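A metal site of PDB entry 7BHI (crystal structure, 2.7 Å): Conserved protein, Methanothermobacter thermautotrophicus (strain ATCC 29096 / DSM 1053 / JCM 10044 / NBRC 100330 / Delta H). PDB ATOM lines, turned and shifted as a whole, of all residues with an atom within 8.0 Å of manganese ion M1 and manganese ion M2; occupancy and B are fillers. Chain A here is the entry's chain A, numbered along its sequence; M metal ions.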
ATOM      1  N   SER A  42     -11.197  13.916 -10.472  1.00  0.00           N
ATOM      2  CA  SER A  42     -11.688  14.537 -11.696  1.00  0.00           C
ATOM      3  C   SER A  42     -10.924  15.782 -12.066  1.00  0.00           C
ATOM      4  O   SER A  42     -10.103  16.292 -11.318  1.00  0.00           O
ATOM      5  CB  SER A  42     -13.191  14.836 -11.540  1.00  0.00           C
ATOM      6  OG  SER A  42     -13.761  15.182 -12.780  1.00  0.00           O
ATOM      7  N   HIS A  43     -11.224  16.262 -13.271  1.00  0.00           N
ATOM      8  CA  HIS A  43     -10.556  17.384 -13.891  1.00  0.00           C
ATOM      9  C   HIS A  43     -11.203  18.704 -13.450  1.00  0.00           C
ATOM     10  O   HIS A  43     -12.275  18.686 -12.845  1.00  0.00           O
ATOM     11  CB  HIS A  43     -10.653  17.189 -15.404  1.00  0.00           C
ATOM     12  CG  HIS A  43      -9.665  17.992 -16.171  1.00  0.00           C
ATOM     13  ND1 HIS A  43     -10.029  18.731 -17.277  1.00  0.00           N
ATOM     14  CD2 HIS A  43      -8.333  18.190 -15.998  1.00  0.00           C
ATOM     15  CE1 HIS A  43      -8.968  19.356 -17.742  1.00  0.00           C
ATOM     16  NE2 HIS A  43      -7.926  19.055 -16.982  1.00  0.00           N
ATOM     17  N   ASN A  44     -10.555  19.822 -13.777  1.00  0.00           N
ATOM     18  CA  ASN A  44     -10.868  21.123 -13.179  1.00  0.00           C
ATOM     19  C   ASN A  44     -11.534  22.157 -14.094  1.00  0.00           C
ATOM     20  O   ASN A  44     -11.332  23.366 -13.920  1.00  0.00           O
ATOM     21  CB  ASN A  44      -9.586  21.724 -12.581  1.00  0.00           C
ATOM     22  CG  ASN A  44      -8.624  22.302 -13.619  1.00  0.00           C
ATOM     23  OD1 ASN A  44      -8.715  22.030 -14.801  1.00  0.00           O
ATOM     24  ND2 ASN A  44      -7.687  23.098 -13.153  1.00  0.00           N
ATOM     25  N   ASP A  45     -12.299  21.672 -15.069  1.00  0.00           N
ATOM     26  CA  ASP A  45     -13.177  22.514 -15.895  1.00  0.00           C
ATOM     27  C   ASP A  45     -14.646  22.046 -15.748  1.00  0.00           C
ATOM     28  O   ASP A  45     -14.926  21.098 -15.022  1.00  0.00           O
ATOM     29  CB  ASP A  45     -12.701  22.550 -17.360  1.00  0.00           C
ATOM     30  CG  ASP A  45     -12.420  21.171 -17.949  1.00  0.00           C
ATOM     31  OD1 ASP A  45     -12.798  20.144 -17.334  1.00  0.00           O
ATOM     32  OD2 ASP A  45     -11.803  21.130 -19.064  1.00  0.00           O
ATOM     33  N   ALA A  46     -15.574  22.730 -16.426  1.00  0.00           N
ATOM     34  CA  ALA A  46     -16.986  22.370 -16.383  1.00  0.00           C
ATOM     35  C   ALA A  46     -17.306  20.873 -16.575  1.00  0.00           C
ATOM     36  O   ALA A  46     -18.114  20.340 -15.848  1.00  0.00           O
ATOM     37  CB  ALA A  46     -17.769  23.195 -17.379  1.00  0.00           C
ATOM     38  N   ASP A  47     -16.664  20.191 -17.537  1.00  0.00           N
ATOM     39  CA  ASP A  47     -16.870  18.745 -17.770  1.00  0.00           C
ATOM     40  C   ASP A  47     -16.424  17.890 -16.595  1.00  0.00           C
ATOM     41  O   ASP A  47     -17.164  17.043 -16.119  1.00  0.00           O
ATOM     42  CB  ASP A  47     -16.142  18.301 -19.044  1.00  0.00           C
ATOM     43  CG  ASP A  47     -16.447  16.863 -19.439  1.00  0.00           C
ATOM     44  OD1 ASP A  47     -17.539  16.340 -19.151  1.00  0.00           O
ATOM     45  OD2 ASP A  47     -15.596  16.230 -20.113  1.00  0.00           O
ATOM     46  N   GLY A  48     -15.196  18.122 -16.144  1.00  0.00           N
ATOM     47  CA  GLY A  48     -14.610  17.453 -14.989  1.00  0.00           C
ATOM     48  C   GLY A  48     -15.395  17.713 -13.714  1.00  0.00           C
ATOM     49  O   GLY A  48     -15.732  16.767 -12.995  1.00  0.00           O
ATOM     50  N   LEU A  49     -15.687  18.978 -13.426  1.00  0.00           N
ATOM     51  CA  LEU A  49     -16.442  19.320 -12.231  1.00  0.00           C
ATOM     52  C   LEU A  49     -17.846  18.724 -12.240  1.00  0.00           C
ATOM     53  O   LEU A  49     -18.260  18.088 -11.267  1.00  0.00           O
ATOM     54  CB  LEU A  49     -16.562  20.842 -12.045  1.00  0.00           C
ATOM     55  CG  LEU A  49     -15.299  21.651 -11.748  1.00  0.00           C
ATOM     56  CD1 LEU A  49     -15.696  23.121 -11.638  1.00  0.00           C
ATOM     57  CD2 LEU A  49     -14.633  21.191 -10.473  1.00  0.00           C
ATOM     58  N   ALA A  51     -18.933  16.219 -14.020  1.00  0.00           N
ATOM     59  CA  ALA A  51     -18.839  14.743 -14.007  1.00  0.00           C
ATOM     60  C   ALA A  51     -18.723  14.172 -12.583  1.00  0.00           C
ATOM     61  O   ALA A  51     -19.495  13.302 -12.207  1.00  0.00           O
ATOM     62  CB  ALA A  51     -17.667  14.271 -14.841  1.00  0.00           C
ATOM     63  N   LEU A  71      -8.063  17.959  -9.993  1.00  0.00           N
ATOM     64  CA  LEU A  71      -6.690  18.181 -10.478  1.00  0.00           C
ATOM     65  C   LEU A  71      -6.727  18.902 -11.809  1.00  0.00           C
ATOM     66  O   LEU A  71      -7.669  18.741 -12.568  1.00  0.00           O
ATOM     67  CB  LEU A  71      -5.995  16.835 -10.717  1.00  0.00           C
ATOM     68  CG  LEU A  71      -6.133  15.755  -9.637  1.00  0.00           C
ATOM     69  CD1 LEU A  71      -5.543  14.437 -10.137  1.00  0.00           C
ATOM     70  CD2 LEU A  71      -5.447  16.200  -8.348  1.00  0.00           C
ATOM     71  N   SER A  72      -5.688  19.689 -12.104  1.00  0.00           N
ATOM     72  CA  SER A  72      -5.520  20.280 -13.438  1.00  0.00           C
ATOM     73  C   SER A  72      -4.991  19.238 -14.427  1.00  0.00           C
ATOM     74  O   SER A  72      -5.384  19.209 -15.590  1.00  0.00           O
ATOM     75  CB  SER A  72      -4.576  21.460 -13.392  1.00  0.00           C
ATOM     76  OG  SER A  72      -3.275  21.049 -13.059  1.00  0.00           O
ATOM     77  N   CYS A  93     -12.817  10.742 -13.553  1.00  0.00           N
ATOM     78  CA  CYS A  93     -13.594  11.387 -14.614  1.00  0.00           C
ATOM     79  C   CYS A  93     -12.740  12.328 -15.446  1.00  0.00           C
ATOM     80  O   CYS A  93     -11.903  13.052 -14.914  1.00  0.00           O
ATOM     81  CB  CYS A  93     -14.758  12.155 -14.035  1.00  0.00           C
ATOM     82  SG  CYS A  93     -15.831  11.153 -12.982  1.00  0.00           S
ATOM     83  N   ASP A  94     -12.962  12.295 -16.754  1.00  0.00           N
ATOM     84  CA  ASP A  94     -12.351  13.208 -17.718  1.00  0.00           C
ATOM     85  C   ASP A  94     -10.836  13.057 -17.787  1.00  0.00           C
ATOM     86  O   ASP A  94     -10.141  13.955 -18.276  1.00  0.00           O
ATOM     87  CB  ASP A  94     -12.743  14.648 -17.354  1.00  0.00           C
ATOM     88  CG  ASP A  94     -12.753  15.588 -18.540  1.00  0.00           C
ATOM     89  OD1 ASP A  94     -12.811  15.153 -19.718  1.00  0.00           O
ATOM     90  OD2 ASP A  94     -12.708  16.802 -18.255  1.00  0.00           O
ATOM     91  N   MET A  95     -10.330  11.908 -17.325  1.00  0.00           N
ATOM     92  CA  MET A  95      -8.920  11.562 -17.320  1.00  0.00           C
ATOM     93  C   MET A  95      -8.796  10.104 -16.877  1.00  0.00           C
ATOM     94  O   MET A  95      -9.620   9.624 -16.119  1.00  0.00           O
ATOM     95  CB  MET A  95      -8.121  12.482 -16.392  1.00  0.00           C
ATOM     96  CG  MET A  95      -8.462  12.363 -14.917  1.00  0.00           C
ATOM     97  SD  MET A  95      -7.970  13.799 -13.935  1.00  0.00           S
ATOM     98  CE  MET A  95      -8.203  13.094 -12.321  1.00  0.00           C
ATOM     99  N   ALA A 113     -14.036   6.950 -16.352  1.00  0.00           N
ATOM    100  CA  ALA A 113     -15.017   7.597 -17.208  1.00  0.00           C
ATOM    101  C   ALA A 113     -14.396   8.827 -17.908  1.00  0.00           C
ATOM    102  O   ALA A 113     -14.556   9.953 -17.451  1.00  0.00           O
ATOM    103  CB  ALA A 113     -16.235   7.990 -16.383  1.00  0.00           C
ATOM    104  N   ASP A 114     -13.719   8.581 -19.021  1.00  0.00           N
ATOM    105  CA  ASP A 114     -13.040   9.584 -19.835  1.00  0.00           C
ATOM    106  C   ASP A 114     -13.675   9.630 -21.252  1.00  0.00           C
ATOM    107  O   ASP A 114     -14.616   8.887 -21.565  1.00  0.00           O
ATOM    108  CB  ASP A 114     -11.574   9.169 -19.914  1.00  0.00           C
ATOM    109  CG  ASP A 114     -10.610  10.293 -20.294  1.00  0.00           C
ATOM    110  OD1 ASP A 114     -11.023  11.393 -20.774  1.00  0.00           O
ATOM    111  OD2 ASP A 114      -9.385  10.074 -20.126  1.00  0.00           O
ATOM    112  N   HIS A 115     -13.219  10.556 -22.084  1.00  0.00           N
ATOM    113  CA  HIS A 115     -13.602  10.635 -23.485  1.00  0.00           C
ATOM    114  C   HIS A 115     -12.460  11.092 -24.404  1.00  0.00           C
ATOM    115  O   HIS A 115     -12.730  11.449 -25.538  1.00  0.00           O
ATOM    116  CB  HIS A 115     -14.820  11.540 -23.652  1.00  0.00           C
ATOM    117  CG  HIS A 115     -14.582  12.978 -23.324  1.00  0.00           C
ATOM    118  ND1 HIS A 115     -14.838  14.007 -24.223  1.00  0.00           N
ATOM    119  CD2 HIS A 115     -14.131  13.578 -22.198  1.00  0.00           C
ATOM    120  CE1 HIS A 115     -14.531  15.162 -23.667  1.00  0.00           C
ATOM    121  NE2 HIS A 115     -14.105  14.927 -22.430  1.00  0.00           N
ATOM    122  N   HIS A 116     -11.209  11.050 -23.951  1.00  0.00           N
ATOM    123  CA  HIS A 116     -10.052  11.475 -24.743  1.00  0.00           C
ATOM    124  C   HIS A 116      -9.501  10.272 -25.499  1.00  0.00           C
ATOM    125  O   HIS A 116      -9.827   9.126 -25.150  1.00  0.00           O
ATOM    126  CB  HIS A 116      -8.966  12.058 -23.832  1.00  0.00           C
ATOM    127  CG  HIS A 116      -9.367  13.318 -23.146  1.00  0.00           C
ATOM    128  ND1 HIS A 116      -9.325  13.470 -21.781  1.00  0.00           N
ATOM    129  CD2 HIS A 116      -9.862  14.479 -23.641  1.00  0.00           C
ATOM    130  CE1 HIS A 116      -9.757  14.689 -21.465  1.00  0.00           C
ATOM    131  NE2 HIS A 116     -10.085  15.312 -22.573  1.00  0.00           N
ATOM    132  N   GLY A 139     -15.827  11.078 -29.185  1.00  0.00           N
ATOM    133  CA  GLY A 139     -15.662  11.734 -27.890  1.00  0.00           C
ATOM    134  C   GLY A 139     -15.342  13.226 -27.937  1.00  0.00           C
ATOM    135  O   GLY A 139     -15.242  13.846 -26.891  1.00  0.00           O
ATOM    136  N   LEU A 143     -19.984  13.049 -26.865  1.00  0.00           N
ATOM    137  CA  LEU A 143     -20.025  12.579 -25.474  1.00  0.00           C
ATOM    138  C   LEU A 143     -18.814  13.069 -24.677  1.00  0.00           C
ATOM    139  O   LEU A 143     -17.659  12.868 -25.080  1.00  0.00           O
ATOM    140  CB  LEU A 143     -20.118  11.046 -25.414  1.00  0.00           C
ATOM    141  CG  LEU A 143     -20.381  10.405 -24.054  1.00  0.00           C
ATOM    142  CD1 LEU A 143     -21.713  10.830 -23.477  1.00  0.00           C
ATOM    143  CD2 LEU A 143     -20.305   8.900 -24.144  1.00  0.00           C
ATOM    144  N   SER A 144     -19.083  13.721 -23.549  1.00  0.00           N
ATOM    145  CA  SER A 144     -18.061  14.223 -22.622  1.00  0.00           C
ATOM    146  C   SER A 144     -17.987  13.347 -21.371  1.00  0.00           C
ATOM    147  O   SER A 144     -18.793  12.419 -21.190  1.00  0.00           O
ATOM    148  CB  SER A 144     -18.369  15.680 -22.244  1.00  0.00           C
ATOM    149  OG  SER A 144     -19.354  15.771 -21.233  1.00  0.00           O
ATOM    150  N   ALA A 145     -17.006  13.645 -20.522  1.00  0.00           N
ATOM    151  CA  ALA A 145     -16.818  12.889 -19.283  1.00  0.00           C
ATOM    152  C   ALA A 145     -18.086  12.869 -18.445  1.00  0.00           C
ATOM    153  O   ALA A 145     -18.400  11.876 -17.820  1.00  0.00           O
ATOM    154  CB  ALA A 145     -15.677  13.479 -18.467  1.00  0.00           C
ATOM    155  N   SER A 146     -18.795  13.992 -18.407  1.00  0.00           N
ATOM    156  CA  SER A 146     -20.011  14.098 -17.608  1.00  0.00           C
ATOM    157  C   SER A 146     -21.103  13.115 -18.070  1.00  0.00           C
ATOM    158  O   SER A 146     -21.704  12.440 -17.244  1.00  0.00           O
ATOM    159  CB  SER A 146     -20.512  15.547 -17.630  1.00  0.00           C
ATOM    160  OG  SER A 146     -20.993  15.847 -18.907  1.00  0.00           O
ATOM    161  N   GLY A 167     -21.515  19.601 -18.578  1.00  0.00           N
ATOM    162  CA  GLY A 167     -20.185  19.198 -19.006  1.00  0.00           C
ATOM    163  C   GLY A 167     -20.041  19.175 -20.503  1.00  0.00           C
ATOM    164  O   GLY A 167     -19.023  19.634 -21.030  1.00  0.00           O
ATOM    165  N   ALA A 168     -21.069  18.655 -21.203  1.00  0.00           N
ATOM    166  CA  ALA A 168     -21.139  18.634 -22.669  1.00  0.00           C
ATOM    167  C   ALA A 168     -20.986  20.024 -23.238  1.00  0.00           C
ATOM    168  O   ALA A 168     -20.137  20.255 -24.105  1.00  0.00           O
ATOM    169  CB  ALA A 168     -22.453  18.037 -23.134  1.00  0.00           C
ATOM    170  N   GLY A 170     -19.862  22.569 -21.586  1.00  0.00           N
ATOM    171  CA  GLY A 170     -18.540  22.984 -21.114  1.00  0.00           C
ATOM    172  C   GLY A 170     -17.455  22.747 -22.137  1.00  0.00           C
ATOM    173  O   GLY A 170     -16.695  23.652 -22.444  1.00  0.00           O
ATOM    174  N   ASP A 171     -17.433  21.538 -22.695  1.00  0.00           N
ATOM    175  CA  ASP A 171     -16.492  21.157 -23.743  1.00  0.00           C
ATOM    176  C   ASP A 171     -17.023  21.396 -25.181  1.00  0.00           C
ATOM    177  O   ASP A 171     -16.563  20.764 -26.125  1.00  0.00           O
ATOM    178  CB  ASP A 171     -16.082  19.683 -23.557  1.00  0.00           C
ATOM    179  CG  ASP A 171     -15.148  19.469 -22.366  1.00  0.00           C
ATOM    180  OD1 ASP A 171     -14.836  20.449 -21.636  1.00  0.00           O
ATOM    181  OD2 ASP A 171     -14.701  18.313 -22.181  1.00  0.00           O
ATOM    182  N   GLN A 173     -19.556  20.533 -27.056  1.00  0.00           N
ATOM    183  CA  GLN A 173     -20.143  19.453 -27.837  1.00  0.00           C
ATOM    184  C   GLN A 173     -21.572  19.823 -28.300  1.00  0.00           C
ATOM    185  O   GLN A 173     -22.516  19.028 -28.215  1.00  0.00           O
ATOM    186  CB  GLN A 173     -20.176  18.175 -27.024  1.00  0.00           C
ATOM    187  CG  GLN A 173     -18.839  17.783 -26.459  1.00  0.00           C
ATOM    188  CD  GLN A 173     -18.783  16.325 -26.031  1.00  0.00           C
ATOM    189  OE1 GLN A 173     -19.790  15.740 -25.657  1.00  0.00           O
ATOM    190  NE2 GLN A 173     -17.597  15.740 -26.096  1.00  0.00           N
ATOM    191  N   ASP A 294     -16.874  26.861 -15.006  1.00  0.00           N
ATOM    192  CA  ASP A 294     -15.567  27.153 -15.632  1.00  0.00           C
ATOM    193  C   ASP A 294     -14.849  28.252 -14.870  1.00  0.00           C
ATOM    194  O   ASP A 294     -13.664  28.127 -14.546  1.00  0.00           O
ATOM    195  CB  ASP A 294     -15.720  27.573 -17.118  1.00  0.00           C
ATOM    196  CG  ASP A 294     -15.758  26.374 -18.085  1.00  0.00           C
ATOM    197  OD1 ASP A 294     -14.953  25.406 -17.920  1.00  0.00           O
ATOM    198  OD2 ASP A 294     -16.581  26.402 -19.025  1.00  0.00           O
HETATM  199 MN    MN M   1     -13.735  16.729 -21.022  1.00  0.00          MN
HETATM  200 MN    MN M   2     -12.004  18.609 -19.079  1.00  0.00          MN
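O of Ala 113 lies within hydrogen-bond range of N of Asp 94 (2.9 Å). The backbone NH of Ala 145 sits at hydrogen-bond distance from the side-chain carboxylate of Asp 47 (3.1 Å). The side-chain hydroxyl (OG) of Ser 144 sits at hydrogen-bond distance from the side-chain carboxylate (OD1) of Asp 47 (2.8 Å). OD1 of Asp 47 sits at hydrogen-bond distance from N of Ser 146, 2.8 Å away. A ring nitrogen (ND1) of His 115 is in hydrogen-bond range of the backbone carbonyl oxygen of Leu 143, 3.2 Å away. The side-chain carboxylate (OD1) of Asp 45 lies close to the backbone NH (N) of Gly 48 (3.4 Å). O of His 43 is in hydrogen-bond range of N of Leu 49 (3.5 Å). A ring nitrogen (NE2) of His 43 sits at hydrogen-bond distance from the backbone carbonyl oxygen (O) of Ser 72, at 2.9 Å.
Three residues have an atom within 4 Å of manganese ion M2: His 43, Asp 45 and Asp 94. The nearest printed residue that does not touch manganese ion M2 is Asp 171 (4.1 Å).
Manganese ion M1 is bound by the side-chain carboxylate (OD2) of Asp 47 (2.1 Å), the side-chain carboxylate (OD2) of Asp 171 (2.2 Å), the side-chain carboxylate (OD1) of Asp 94 (2.2 Å) and a ring nitrogen (NE2) of His 115 (2.3 Å). Manganese ion M1 has four donor atoms within binding distance.
Manganese ion M2 is bound by OD2 of Asp 94 (2.1 Å). Manganese ion M2 is bound by the side-chain carboxylate (OD1) of Asp 45 (2.5 Å). OD2 of Asp 45 binds manganese ion M2 (2.5 Å). Manganese ion M2 is bound by ND1 of His 43, 2.7 Å away. Manganese ion M2 has four donor atoms within binding distance.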
